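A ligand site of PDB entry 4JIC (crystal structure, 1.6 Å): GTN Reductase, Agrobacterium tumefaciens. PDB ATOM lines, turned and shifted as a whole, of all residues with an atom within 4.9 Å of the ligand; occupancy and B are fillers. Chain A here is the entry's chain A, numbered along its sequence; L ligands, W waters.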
ATOM      1  N   ALA A  22      -9.354 -10.548   5.582  1.00  0.00           N
ATOM      2  CA  ALA A  22      -9.290 -10.520   4.132  1.00  0.00           C
ATOM      3  C   ALA A  22     -10.340 -11.463   3.549  1.00  0.00           C
ATOM      4  O   ALA A  22     -10.743 -12.426   4.210  1.00  0.00           O
ATOM      5  CB  ALA A  22      -7.898 -10.912   3.673  1.00  0.00           C
ATOM      6  N   PRO A  23     -10.786 -11.194   2.327  1.00  0.00           N
ATOM      7  CA  PRO A  23     -11.749 -12.061   1.643  1.00  0.00           C
ATOM      8  C   PRO A  23     -11.119 -13.423   1.353  1.00  0.00           C
ATOM      9  O   PRO A  23     -10.009 -13.509   0.835  1.00  0.00           O
ATOM     10  CB  PRO A  23     -12.050 -11.304   0.346  1.00  0.00           C
ATOM     11  CG  PRO A  23     -10.840 -10.420   0.134  1.00  0.00           C
ATOM     12  CD  PRO A  23     -10.356 -10.050   1.492  1.00  0.00           C
ATOM     13  N   LEU A  24     -11.818 -14.491   1.705  1.00  0.00           N
ATOM     14  CA  LEU A  24     -11.279 -15.839   1.563  1.00  0.00           C
ATOM     15  C   LEU A  24     -12.346 -16.789   1.040  1.00  0.00           C
ATOM     16  O   LEU A  24     -13.225 -17.212   1.791  1.00  0.00           O
ATOM     17  CB  LEU A  24     -10.745 -16.356   2.912  1.00  0.00           C
ATOM     18  CG  LEU A  24      -9.637 -15.536   3.571  1.00  0.00           C
ATOM     19  CD1 LEU A  24      -9.699 -15.719   5.100  1.00  0.00           C
ATOM     20  CD2 LEU A  24      -8.260 -15.911   3.019  1.00  0.00           C
ATOM     21  N   THR A  25     -12.242 -17.129  -0.238  1.00  0.00           N
ATOM     22  CA  THR A  25     -13.101 -18.149  -0.843  1.00  0.00           C
ATOM     23  C   THR A  25     -12.895 -19.477  -0.136  1.00  0.00           C
ATOM     24  O   THR A  25     -11.768 -19.960  -0.021  1.00  0.00           O
ATOM     25  CB  THR A  25     -12.735 -18.315  -2.328  1.00  0.00           C
ATOM     26  OG1 THR A  25     -13.081 -17.117  -3.068  1.00  0.00           O
ATOM     27  CG2 THR A  25     -13.447 -19.504  -2.942  1.00  0.00           C
ATOM     28  N   ARG A  26     -13.990 -20.086   0.347  1.00  0.00           N
ATOM     29  CA  ARG A  26     -13.897 -21.355   1.077  1.00  0.00           C
ATOM     30  C   ARG A  26     -14.724 -22.499   0.448  1.00  0.00           C
ATOM     31  O   ARG A  26     -14.594 -23.661   0.845  1.00  0.00           O
ATOM     32  CB  ARG A  26     -14.311 -21.171   2.554  1.00  0.00           C
ATOM     33  CG  ARG A  26     -13.605 -20.032   3.310  1.00  0.00           C
ATOM     34  CD  ARG A  26     -12.093 -20.160   3.300  1.00  0.00           C
ATOM     35  NE  ARG A  26     -11.620 -21.431   3.840  1.00  0.00           N
ATOM     36  CZ  ARG A  26     -11.445 -21.678   5.130  1.00  0.00           C
ATOM     37  NH1 ARG A  26     -10.998 -22.872   5.525  1.00  0.00           N
ATOM     38  NH2 ARG A  26     -11.712 -20.746   6.042  1.00  0.00           N
ATOM     39  N   GLU A  54     -15.715 -13.809   1.826  1.00  0.00           N
ATOM     40  CA  GLU A  54     -15.341 -14.535   0.617  1.00  0.00           C
ATOM     41  C   GLU A  54     -15.979 -13.858  -0.582  1.00  0.00           C
ATOM     42  O   GLU A  54     -17.069 -13.305  -0.483  1.00  0.00           O
ATOM     43  CB  GLU A  54     -15.861 -15.974   0.712  1.00  0.00           C
ATOM     44  CG  GLU A  54     -17.383 -16.090   0.797  1.00  0.00           C
ATOM     45  CD  GLU A  54     -17.792 -17.367   1.516  1.00  0.00           C
ATOM     46  OE1 GLU A  54     -17.793 -18.445   0.877  1.00  0.00           O
ATOM     47  OE2 GLU A  54     -18.096 -17.293   2.735  1.00  0.00           O
ATOM     48  N   GLY A  55     -15.315 -13.899  -1.731  1.00  0.00           N
ATOM     49  CA  GLY A  55     -15.935 -13.390  -2.941  1.00  0.00           C
ATOM     50  C   GLY A  55     -17.347 -13.947  -3.073  1.00  0.00           C
ATOM     51  O   GLY A  55     -17.576 -15.143  -2.951  1.00  0.00           O
ATOM     52  N   GLN A  97     -17.896  -8.935  -0.421  1.00  0.00           N
ATOM     53  CA  GLN A  97     -17.005  -8.740  -1.562  1.00  0.00           C
ATOM     54  C   GLN A  97     -17.732  -9.140  -2.827  1.00  0.00           C
ATOM     55  O   GLN A  97     -17.771 -10.304  -3.203  1.00  0.00           O
ATOM     56  CB  GLN A  97     -15.719  -9.556  -1.454  1.00  0.00           C
ATOM     57  CG  GLN A  97     -14.736  -9.098  -2.515  1.00  0.00           C
ATOM     58  CD  GLN A  97     -13.518  -9.961  -2.648  1.00  0.00           C
ATOM     59  OE1 GLN A  97     -13.626 -11.180  -2.772  1.00  0.00           O
ATOM     60  NE2 GLN A  97     -12.346  -9.335  -2.685  1.00  0.00           N
ATOM     61  N   TRP A  99     -18.640  -9.885  -6.480  1.00  0.00           N
ATOM     62  CA  TRP A  99     -17.664 -10.511  -7.364  1.00  0.00           C
ATOM     63  C   TRP A  99     -18.220 -10.790  -8.737  1.00  0.00           C
ATOM     64  O   TRP A  99     -19.385 -11.179  -8.886  1.00  0.00           O
ATOM     65  CB  TRP A  99     -17.283 -11.844  -6.739  1.00  0.00           C
ATOM     66  CG  TRP A  99     -16.018 -12.518  -7.181  1.00  0.00           C
ATOM     67  CD1 TRP A  99     -14.996 -12.007  -7.969  1.00  0.00           C
ATOM     68  CD2 TRP A  99     -15.617 -13.836  -6.808  1.00  0.00           C
ATOM     69  NE1 TRP A  99     -14.006 -12.962  -8.107  1.00  0.00           N
ATOM     70  CE2 TRP A  99     -14.370 -14.089  -7.410  1.00  0.00           C
ATOM     71  CE3 TRP A  99     -16.209 -14.840  -6.042  1.00  0.00           C
ATOM     72  CZ2 TRP A  99     -13.696 -15.306  -7.239  1.00  0.00           C
ATOM     73  CZ3 TRP A  99     -15.552 -16.030  -5.873  1.00  0.00           C
ATOM     74  CH2 TRP A  99     -14.310 -16.263  -6.468  1.00  0.00           C
ATOM     75  N   HIS A 178     -14.866  -6.413  -5.831  1.00  0.00           N
ATOM     76  CA  HIS A 178     -13.710  -7.226  -6.199  1.00  0.00           C
ATOM     77  C   HIS A 178     -13.152  -6.772  -7.551  1.00  0.00           C
ATOM     78  O   HIS A 178     -13.686  -7.108  -8.600  1.00  0.00           O
ATOM     79  CB  HIS A 178     -14.095  -8.709  -6.249  1.00  0.00           C
ATOM     80  CG  HIS A 178     -12.916  -9.630  -6.171  1.00  0.00           C
ATOM     81  ND1 HIS A 178     -11.651  -9.243  -6.520  1.00  0.00           N
ATOM     82  CD2 HIS A 178     -12.827 -10.921  -5.763  1.00  0.00           C
ATOM     83  CE1 HIS A 178     -10.818 -10.254  -6.338  1.00  0.00           C
ATOM     84  NE2 HIS A 178     -11.510 -11.293  -5.888  1.00  0.00           N
ATOM     85  N   ASN A 181      -7.082  -9.622  -8.527  1.00  0.00           N
ATOM     86  CA  ASN A 181      -6.761 -11.029  -8.757  1.00  0.00           C
ATOM     87  C   ASN A 181      -7.196 -11.602 -10.105  1.00  0.00           C
ATOM     88  O   ASN A 181      -7.617 -12.754 -10.200  1.00  0.00           O
ATOM     89  CB  ASN A 181      -7.265 -11.898  -7.595  1.00  0.00           C
ATOM     90  CG  ASN A 181      -6.650 -11.474  -6.278  1.00  0.00           C
ATOM     91  OD1 ASN A 181      -5.550 -10.929  -6.246  1.00  0.00           O
ATOM     92  ND2 ASN A 181      -7.356 -11.731  -5.175  1.00  0.00           N
ATOM     93  N   ARG A 230     -11.245  -3.492  -3.947  1.00  0.00           N
ATOM     94  CA  ARG A 230      -9.962  -4.165  -3.794  1.00  0.00           C
ATOM     95  C   ARG A 230      -9.180  -4.129  -5.095  1.00  0.00           C
ATOM     96  O   ARG A 230      -9.710  -4.441  -6.165  1.00  0.00           O
ATOM     97  CB  ARG A 230     -10.134  -5.625  -3.360  1.00  0.00           C
ATOM     98  CG  ARG A 230      -8.816  -6.192  -2.816  1.00  0.00           C
ATOM     99  CD  ARG A 230      -8.952  -7.621  -2.302  1.00  0.00           C
ATOM    100  NE  ARG A 230      -8.060  -7.846  -1.159  1.00  0.00           N
ATOM    101  CZ  ARG A 230      -7.566  -9.028  -0.809  1.00  0.00           C
ATOM    102  NH1 ARG A 230      -7.830 -10.111  -1.520  1.00  0.00           N
ATOM    103  NH2 ARG A 230      -6.780  -9.116   0.259  1.00  0.00           N
ATOM    104  N   VAL A 267      -3.795  -5.243  -2.444  1.00  0.00           N
ATOM    105  CA  VAL A 267      -2.939  -6.414  -2.367  1.00  0.00           C
ATOM    106  C   VAL A 267      -1.555  -5.975  -2.824  1.00  0.00           C
ATOM    107  O   VAL A 267      -1.369  -5.571  -3.974  1.00  0.00           O
ATOM    108  CB  VAL A 267      -3.437  -7.546  -3.282  1.00  0.00           C
ATOM    109  CG1 VAL A 267      -2.465  -8.719  -3.237  1.00  0.00           C
ATOM    110  CG2 VAL A 267      -4.828  -7.992  -2.861  1.00  0.00           C
ATOM    111  N   THR A 271      -0.451 -12.089  -5.131  1.00  0.00           N
ATOM    112  CA  THR A 271      -1.417 -12.545  -4.121  1.00  0.00           C
ATOM    113  C   THR A 271      -0.954 -13.869  -3.561  1.00  0.00           C
ATOM    114  O   THR A 271      -0.823 -14.850  -4.290  1.00  0.00           O
ATOM    115  CB  THR A 271      -2.808 -12.692  -4.737  1.00  0.00           C
ATOM    116  OG1 THR A 271      -3.099 -11.522  -5.503  1.00  0.00           O
ATOM    117  CG2 THR A 271      -3.858 -12.860  -3.634  1.00  0.00           C
ATOM    118  N   GLY A 272      -0.697 -13.896  -2.251  1.00  0.00           N
ATOM    119  CA  GLY A 272      -0.175 -15.091  -1.612  1.00  0.00           C
ATOM    120  C   GLY A 272       1.290 -15.373  -1.891  1.00  0.00           C
ATOM    121  O   GLY A 272       1.815 -16.417  -1.473  1.00  0.00           O
ATOM    122  N   ASN A 305      -2.820  -5.424   2.351  1.00  0.00           N
ATOM    123  CA  ASN A 305      -2.813  -6.870   2.484  1.00  0.00           C
ATOM    124  C   ASN A 305      -1.593  -7.477   1.794  1.00  0.00           C
ATOM    125  O   ASN A 305      -1.025  -6.884   0.875  1.00  0.00           O
ATOM    126  CB  ASN A 305      -4.075  -7.467   1.855  1.00  0.00           C
ATOM    127  CG  ASN A 305      -3.971  -8.970   1.662  1.00  0.00           C
ATOM    128  OD1 ASN A 305      -3.673  -9.447   0.565  1.00  0.00           O
ATOM    129  ND2 ASN A 305      -4.196  -9.720   2.748  1.00  0.00           N
ATOM    130  N   ASN A 306      -1.229  -8.673   2.277  1.00  0.00           N
ATOM    131  CA  ASN A 306      -0.371  -9.653   1.620  1.00  0.00           C
ATOM    132  C   ASN A 306       0.975  -9.837   2.328  1.00  0.00           C
ATOM    133  O   ASN A 306       1.853  -8.985   2.242  1.00  0.00           O
ATOM    134  CB  ASN A 306      -0.165  -9.401   0.120  1.00  0.00           C
ATOM    135  CG  ASN A 306       0.500 -10.586  -0.561  1.00  0.00           C
ATOM    136  OD1 ASN A 306       0.048 -11.725  -0.395  1.00  0.00           O
ATOM    137  ND2 ASN A 306       1.594 -10.344  -1.275  1.00  0.00           N
ATOM    138  N   GLY A 307       1.099 -10.941   3.039  1.00  0.00           N
ATOM    139  CA  GLY A 307       2.348 -11.261   3.716  1.00  0.00           C
ATOM    140  C   GLY A 307       2.641 -10.502   4.993  1.00  0.00           C
ATOM    141  O   GLY A 307       3.768 -10.521   5.496  1.00  0.00           O
ATOM    142  N   TYR A 308       1.628  -9.829   5.546  1.00  0.00           N
ATOM    143  CA  TYR A 308       1.815  -9.160   6.831  1.00  0.00           C
ATOM    144  C   TYR A 308       1.832 -10.199   7.946  1.00  0.00           C
ATOM    145  O   TYR A 308       1.210 -11.262   7.844  1.00  0.00           O
ATOM    146  CB  TYR A 308       0.692  -8.155   7.094  1.00  0.00           C
ATOM    147  CG  TYR A 308       0.883  -6.858   6.339  1.00  0.00           C
ATOM    148  CD1 TYR A 308       0.318  -6.675   5.082  1.00  0.00           C
ATOM    149  CD2 TYR A 308       1.653  -5.836   6.871  1.00  0.00           C
ATOM    150  CE1 TYR A 308       0.490  -5.493   4.388  1.00  0.00           C
ATOM    151  CE2 TYR A 308       1.832  -4.648   6.180  1.00  0.00           C
ATOM    152  CZ  TYR A 308       1.264  -4.485   4.936  1.00  0.00           C
ATOM    153  OH  TYR A 308       1.449  -3.309   4.252  1.00  0.00           O
ATOM    154  N   ALA A 326      -5.259  -6.139   6.415  1.00  0.00           N
ATOM    155  CA  ALA A 326      -6.095  -7.322   6.223  1.00  0.00           C
ATOM    156  C   ALA A 326      -5.224  -8.568   6.197  1.00  0.00           C
ATOM    157  O   ALA A 326      -4.224  -8.639   5.469  1.00  0.00           O
ATOM    158  CB  ALA A 326      -6.898  -7.208   4.948  1.00  0.00           C
ATOM    159  N   PHE A 327      -5.622  -9.557   6.999  1.00  0.00           N
ATOM    160  CA  PHE A 327      -4.909 -10.823   7.089  1.00  0.00           C
ATOM    161  C   PHE A 327      -5.784 -11.904   6.469  1.00  0.00           C
ATOM    162  O   PHE A 327      -6.980 -11.978   6.765  1.00  0.00           O
ATOM    163  CB  PHE A 327      -4.653 -11.204   8.551  1.00  0.00           C
ATOM    164  CG  PHE A 327      -3.780 -10.246   9.305  1.00  0.00           C
ATOM    165  CD1 PHE A 327      -2.394 -10.401   9.305  1.00  0.00           C
ATOM    166  CD2 PHE A 327      -4.329  -9.191  10.022  1.00  0.00           C
ATOM    167  CE1 PHE A 327      -1.583  -9.534  10.018  1.00  0.00           C
ATOM    168  CE2 PHE A 327      -3.523  -8.313  10.728  1.00  0.00           C
ATOM    169  CZ  PHE A 327      -2.153  -8.483  10.731  1.00  0.00           C
ATOM    170  N   GLY A 328      -5.177 -12.743   5.638  1.00  0.00           N
ATOM    171  CA  GLY A 328      -5.901 -13.825   4.990  1.00  0.00           C
ATOM    172  C   GLY A 328      -5.722 -15.143   5.719  1.00  0.00           C
ATOM    173  O   GLY A 328      -6.564 -15.540   6.527  1.00  0.00           O
ATOM    174  N   LYS A 329      -4.616 -15.825   5.441  1.00  0.00           N
ATOM    175  CA  LYS A 329      -4.410 -17.165   5.970  1.00  0.00           C
ATOM    176  C   LYS A 329      -4.395 -17.208   7.509  1.00  0.00           C
ATOM    177  O   LYS A 329      -4.840 -18.185   8.106  1.00  0.00           O
ATOM    178  CB  LYS A 329      -3.160 -17.790   5.373  1.00  0.00           C
ATOM    179  CG  LYS A 329      -3.297 -18.032   3.873  1.00  0.00           C
ATOM    180  CD  LYS A 329      -2.081 -18.695   3.267  1.00  0.00           C
ATOM    181  CE  LYS A 329      -0.837 -17.854   3.452  1.00  0.00           C
ATOM    182  NZ  LYS A 329      -0.915 -16.604   2.651  1.00  0.00           N
ATOM    183  N   ILE A 332      -7.923 -17.606   8.601  1.00  0.00           N
ATOM    184  CA  ILE A 332      -8.442 -18.960   8.428  1.00  0.00           C
ATOM    185  C   ILE A 332      -8.180 -19.754   9.695  1.00  0.00           C
ATOM    186  O   ILE A 332      -9.065 -20.429  10.216  1.00  0.00           O
ATOM    187  CB  ILE A 332      -7.780 -19.670   7.242  1.00  0.00           C
ATOM    188  CG1 ILE A 332      -8.260 -19.065   5.922  1.00  0.00           C
ATOM    189  CG2 ILE A 332      -8.118 -21.159   7.249  1.00  0.00           C
ATOM    190  CD1 ILE A 332      -7.610 -19.674   4.679  1.00  0.00           C
ATOM    191  N   PHE A 355      -8.434 -25.565   2.906  1.00  0.00           N
ATOM    192  CA  PHE A 355      -8.868 -24.223   2.538  1.00  0.00           C
ATOM    193  C   PHE A 355     -10.168 -24.250   1.730  1.00  0.00           C
ATOM    194  O   PHE A 355     -11.084 -23.487   1.994  1.00  0.00           O
ATOM    195  CB  PHE A 355      -7.790 -23.480   1.750  1.00  0.00           C
ATOM    196  CG  PHE A 355      -6.647 -22.952   2.588  1.00  0.00           C
ATOM    197  CD1 PHE A 355      -6.548 -23.214   3.941  1.00  0.00           C
ATOM    198  CD2 PHE A 355      -5.647 -22.196   1.981  1.00  0.00           C
ATOM    199  CE1 PHE A 355      -5.465 -22.731   4.680  1.00  0.00           C
ATOM    200  CE2 PHE A 355      -4.576 -21.707   2.710  1.00  0.00           C
ATOM    201  CZ  PHE A 355      -4.492 -21.968   4.062  1.00  0.00           C
ATOM    202  N   TYR A 356     -10.219 -25.136   0.729  1.00  0.00           N
ATOM    203  CA  TYR A 356     -11.306 -25.119  -0.256  1.00  0.00           C
ATOM    204  C   TYR A 356     -12.202 -26.342  -0.179  1.00  0.00           C
ATOM    205  O   TYR A 356     -11.726 -27.484  -0.300  1.00  0.00           O
ATOM    206  CB  TYR A 356     -10.707 -25.042  -1.656  1.00  0.00           C
ATOM    207  CG  TYR A 356      -9.758 -23.882  -1.862  1.00  0.00           C
ATOM    208  CD1 TYR A 356     -10.219 -22.578  -1.880  1.00  0.00           C
ATOM    209  CD2 TYR A 356      -8.408 -24.103  -2.085  1.00  0.00           C
ATOM    210  CE1 TYR A 356      -9.356 -21.526  -2.093  1.00  0.00           C
ATOM    211  CE2 TYR A 356      -7.547 -23.064  -2.303  1.00  0.00           C
ATOM    212  CZ  TYR A 356      -8.016 -21.769  -2.315  1.00  0.00           C
ATOM    213  OH  TYR A 356      -7.156 -20.730  -2.534  1.00  0.00           O
HETATM  214  N1  LIG L   1      -8.837 -12.707  -2.360  1.00  0.00           N
HETATM  215  C1  LIG L   1     -10.005 -12.086  -2.727  1.00  0.00           C
HETATM  216  O1  LIG L   1      -9.954 -10.913  -3.113  1.00  0.00           O
HETATM  217  N2  LIG L   1     -11.200 -12.772  -2.684  1.00  0.00           N
HETATM  218  C2  LIG L   1     -11.257 -14.109  -2.384  1.00  0.00           C
HETATM  219  O2  LIG L   1     -12.356 -14.684  -2.363  1.00  0.00           O
HETATM  220  C3  LIG L   1     -10.071 -14.753  -2.024  1.00  0.00           C
HETATM  221  N3  LIG L   1     -10.079 -16.103  -1.725  1.00  0.00           N
HETATM  222  C4  LIG L   1      -8.965 -16.624  -1.097  1.00  0.00           C
HETATM  223  C5  LIG L   1      -9.038 -17.905  -0.551  1.00  0.00           C
HETATM  224  C6  LIG L   1      -7.953 -18.470   0.101  1.00  0.00           C
HETATM  225  C7  LIG L   1      -8.071 -19.848   0.712  1.00  0.00           C
HETATM  226  C8  LIG L   1      -6.786 -17.739   0.223  1.00  0.00           C
HETATM  227  C9  LIG L   1      -5.613 -18.308   0.988  1.00  0.00           C
HETATM  228  C10 LIG L   1      -6.705 -16.443  -0.306  1.00  0.00           C
HETATM  229  C11 LIG L   1      -7.790 -15.884  -0.981  1.00  0.00           C
HETATM  230  N4  LIG L   1      -7.697 -14.613  -1.530  1.00  0.00           N
HETATM  231  C12 LIG L   1      -8.860 -14.044  -2.014  1.00  0.00           C
HETATM  232  C13 LIG L   1      -6.522 -13.723  -1.215  1.00  0.00           C
HETATM  233  C14 LIG L   1      -6.514 -13.252   0.234  1.00  0.00           C
HETATM  234  O3  LIG L   1      -7.561 -12.320   0.465  1.00  0.00           O
HETATM  235  C15 LIG L   1      -5.193 -12.574   0.588  1.00  0.00           C
HETATM  236  O4  LIG L   1      -4.948 -11.546  -0.354  1.00  0.00           O
HETATM  237  C16 LIG L   1      -4.018 -13.541   0.593  1.00  0.00           C
HETATM  238  O5  LIG L   1      -4.298 -14.643   1.427  1.00  0.00           O
HETATM  239  C17 LIG L   1      -2.715 -12.903   1.070  1.00  0.00           C
HETATM  240  O6  LIG L   1      -2.861 -12.397   2.388  1.00  0.00           O
HETATM  241  P1  LIG L   1      -2.159 -13.169   3.632  1.00  0.00           P
HETATM  242  O7  LIG L   1      -2.669 -14.580   3.577  1.00  0.00           O
HETATM  243  O8  LIG L   1      -0.663 -13.124   3.409  1.00  0.00           O
HETATM  244  O9  LIG L   1      -2.552 -12.460   4.886  1.00  0.00           O
HETATM  245  O   HOH W   1       0.890 -14.210   1.635  1.00  0.00           O
HETATM  246  O   HOH W   2      -1.612  -9.866   4.920  1.00  0.00           O
HETATM  247  O   HOH W   3       0.872 -13.163   5.725  1.00  0.00           O
HETATM  248  O   HOH W   4      -2.675 -16.585  -0.019  1.00  0.00           O
HETATM  249  O   HOH W   5      -2.294 -13.856   7.222  1.00  0.00           O
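The side-chain amide oxygen (OD1) of Asn 305 lies within hydrogen-bond range of an oxygen (O4) of the ligand, 2.6 Å away.
N of Thr 25 lies within hydrogen-bond range of N3 of the ligand, 2.8 Å away.
An oxygen (O2) of the ligand is in hydrogen-bond range of the side-chain hydroxyl (OG1) of Thr 25.
The backbone NH (N) of Gly 328 lies within hydrogen-bond range of an oxygen (O9) of the ligand (2.7 Å).
The backbone carbonyl oxygen of Pro 23 lies within hydrogen-bond range of an oxygen (O3) of the ligand, 2.7 Å away.
NH1 of Arg 230 sits at hydrogen-bond distance from O1 of the ligand, 2.8 Å away.
N of Gly 307 is in hydrogen-bond range of O8 of the ligand, at 2.8 Å.
The backbone NH of Lys 329 lies within hydrogen-bond range of an oxygen (O7) of the ligand (3.0 Å).
The side-chain amino group (NZ) of Lys 329 is in salt-bridge range of an oxygen (O7) of the ligand, 2.8 Å away.
The side-chain amide nitrogen (NE2) of Gln 97 lies within hydrogen-bond range of an oxygen (O1) of the ligand, 2.9 Å away.
O2 of the ligand lies within hydrogen-bond range of N of Gly 55 (3.1 Å).
O1 of the ligand sits at hydrogen-bond distance from NE2 of His 178 (3.2 Å).
The side-chain amide nitrogen of Asn 181 sits at hydrogen-bond distance from a nitrogen (N1) of the ligand (3.3 Å).
The side-chain amide oxygen of Asn 305 sits at hydrogen-bond distance from the guanidinium group of Arg 230.
ND2 of Asn 305 is in hydrogen-bond range of O of Ala 326.
The backbone NH (N) of Gly 55 sits close to the side-chain amide oxygen (OE1) of Gln 97 (3.4 Å).
The side-chain amide oxygen (OD1) of Asn 181 is in hydrogen-bond range of the side-chain hydroxyl (OG1) of Thr 271, at 2.6 Å.
OD1 of Asn 306 is in hydrogen-bond range of N of Gly 272.
The backbone NH (N) of Ala 22 is in hydrogen-bond range of the backbone carbonyl oxygen (O) of Phe 327, at 3.0 Å.
NE of Arg 26 sits at hydrogen-bond distance from O of Phe 355, 2.8 Å away.
CB of Ala 22 touches O3 of the ligand, at 3.5 Å.
Leu 24 touches the ligand (CA to N3, 3.5 Å).
Thr 271 touches the ligand.
Asn 306 touches the ligand.
Phe 327 touches the ligand.
Ile 332 touches the ligand.
CD2 of Phe 355 touches C7 of the ligand (3.6 Å).
Tyr 356 touches the ligand.
Hydrophobic or aromatic side chains that line the ligand: Ala 22, Pro 23, Leu 24, His 178, Ile 332, Phe 355 and Tyr 356.
Of the 26 residues printed, 19 come within 4 Å of the ligand.
The nearest printed residue that does not touch the ligand is Gly 272 (4.01 Å).
Water W1 lies within hydrogen-bond range of O8 of the ligand (2.6 Å), NZ of Lys 329 (3.2 Å) and OD1 of Asn 306 (3.3 Å).
Water W5 lies within hydrogen-bond range of O9 of the ligand and N of Gly 328.
Water W3 lies within hydrogen-bond range of an oxygen (O8) of the ligand (2.8 Å), the backbone carbonyl oxygen (O) of Tyr 308 (2.9 Å) and the backbone NH (N) of Gly 307 (3.5 Å).
Water W4 bridges O5 of the ligand (2.9 Å) and NZ of Lys 329 (3.2 Å).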
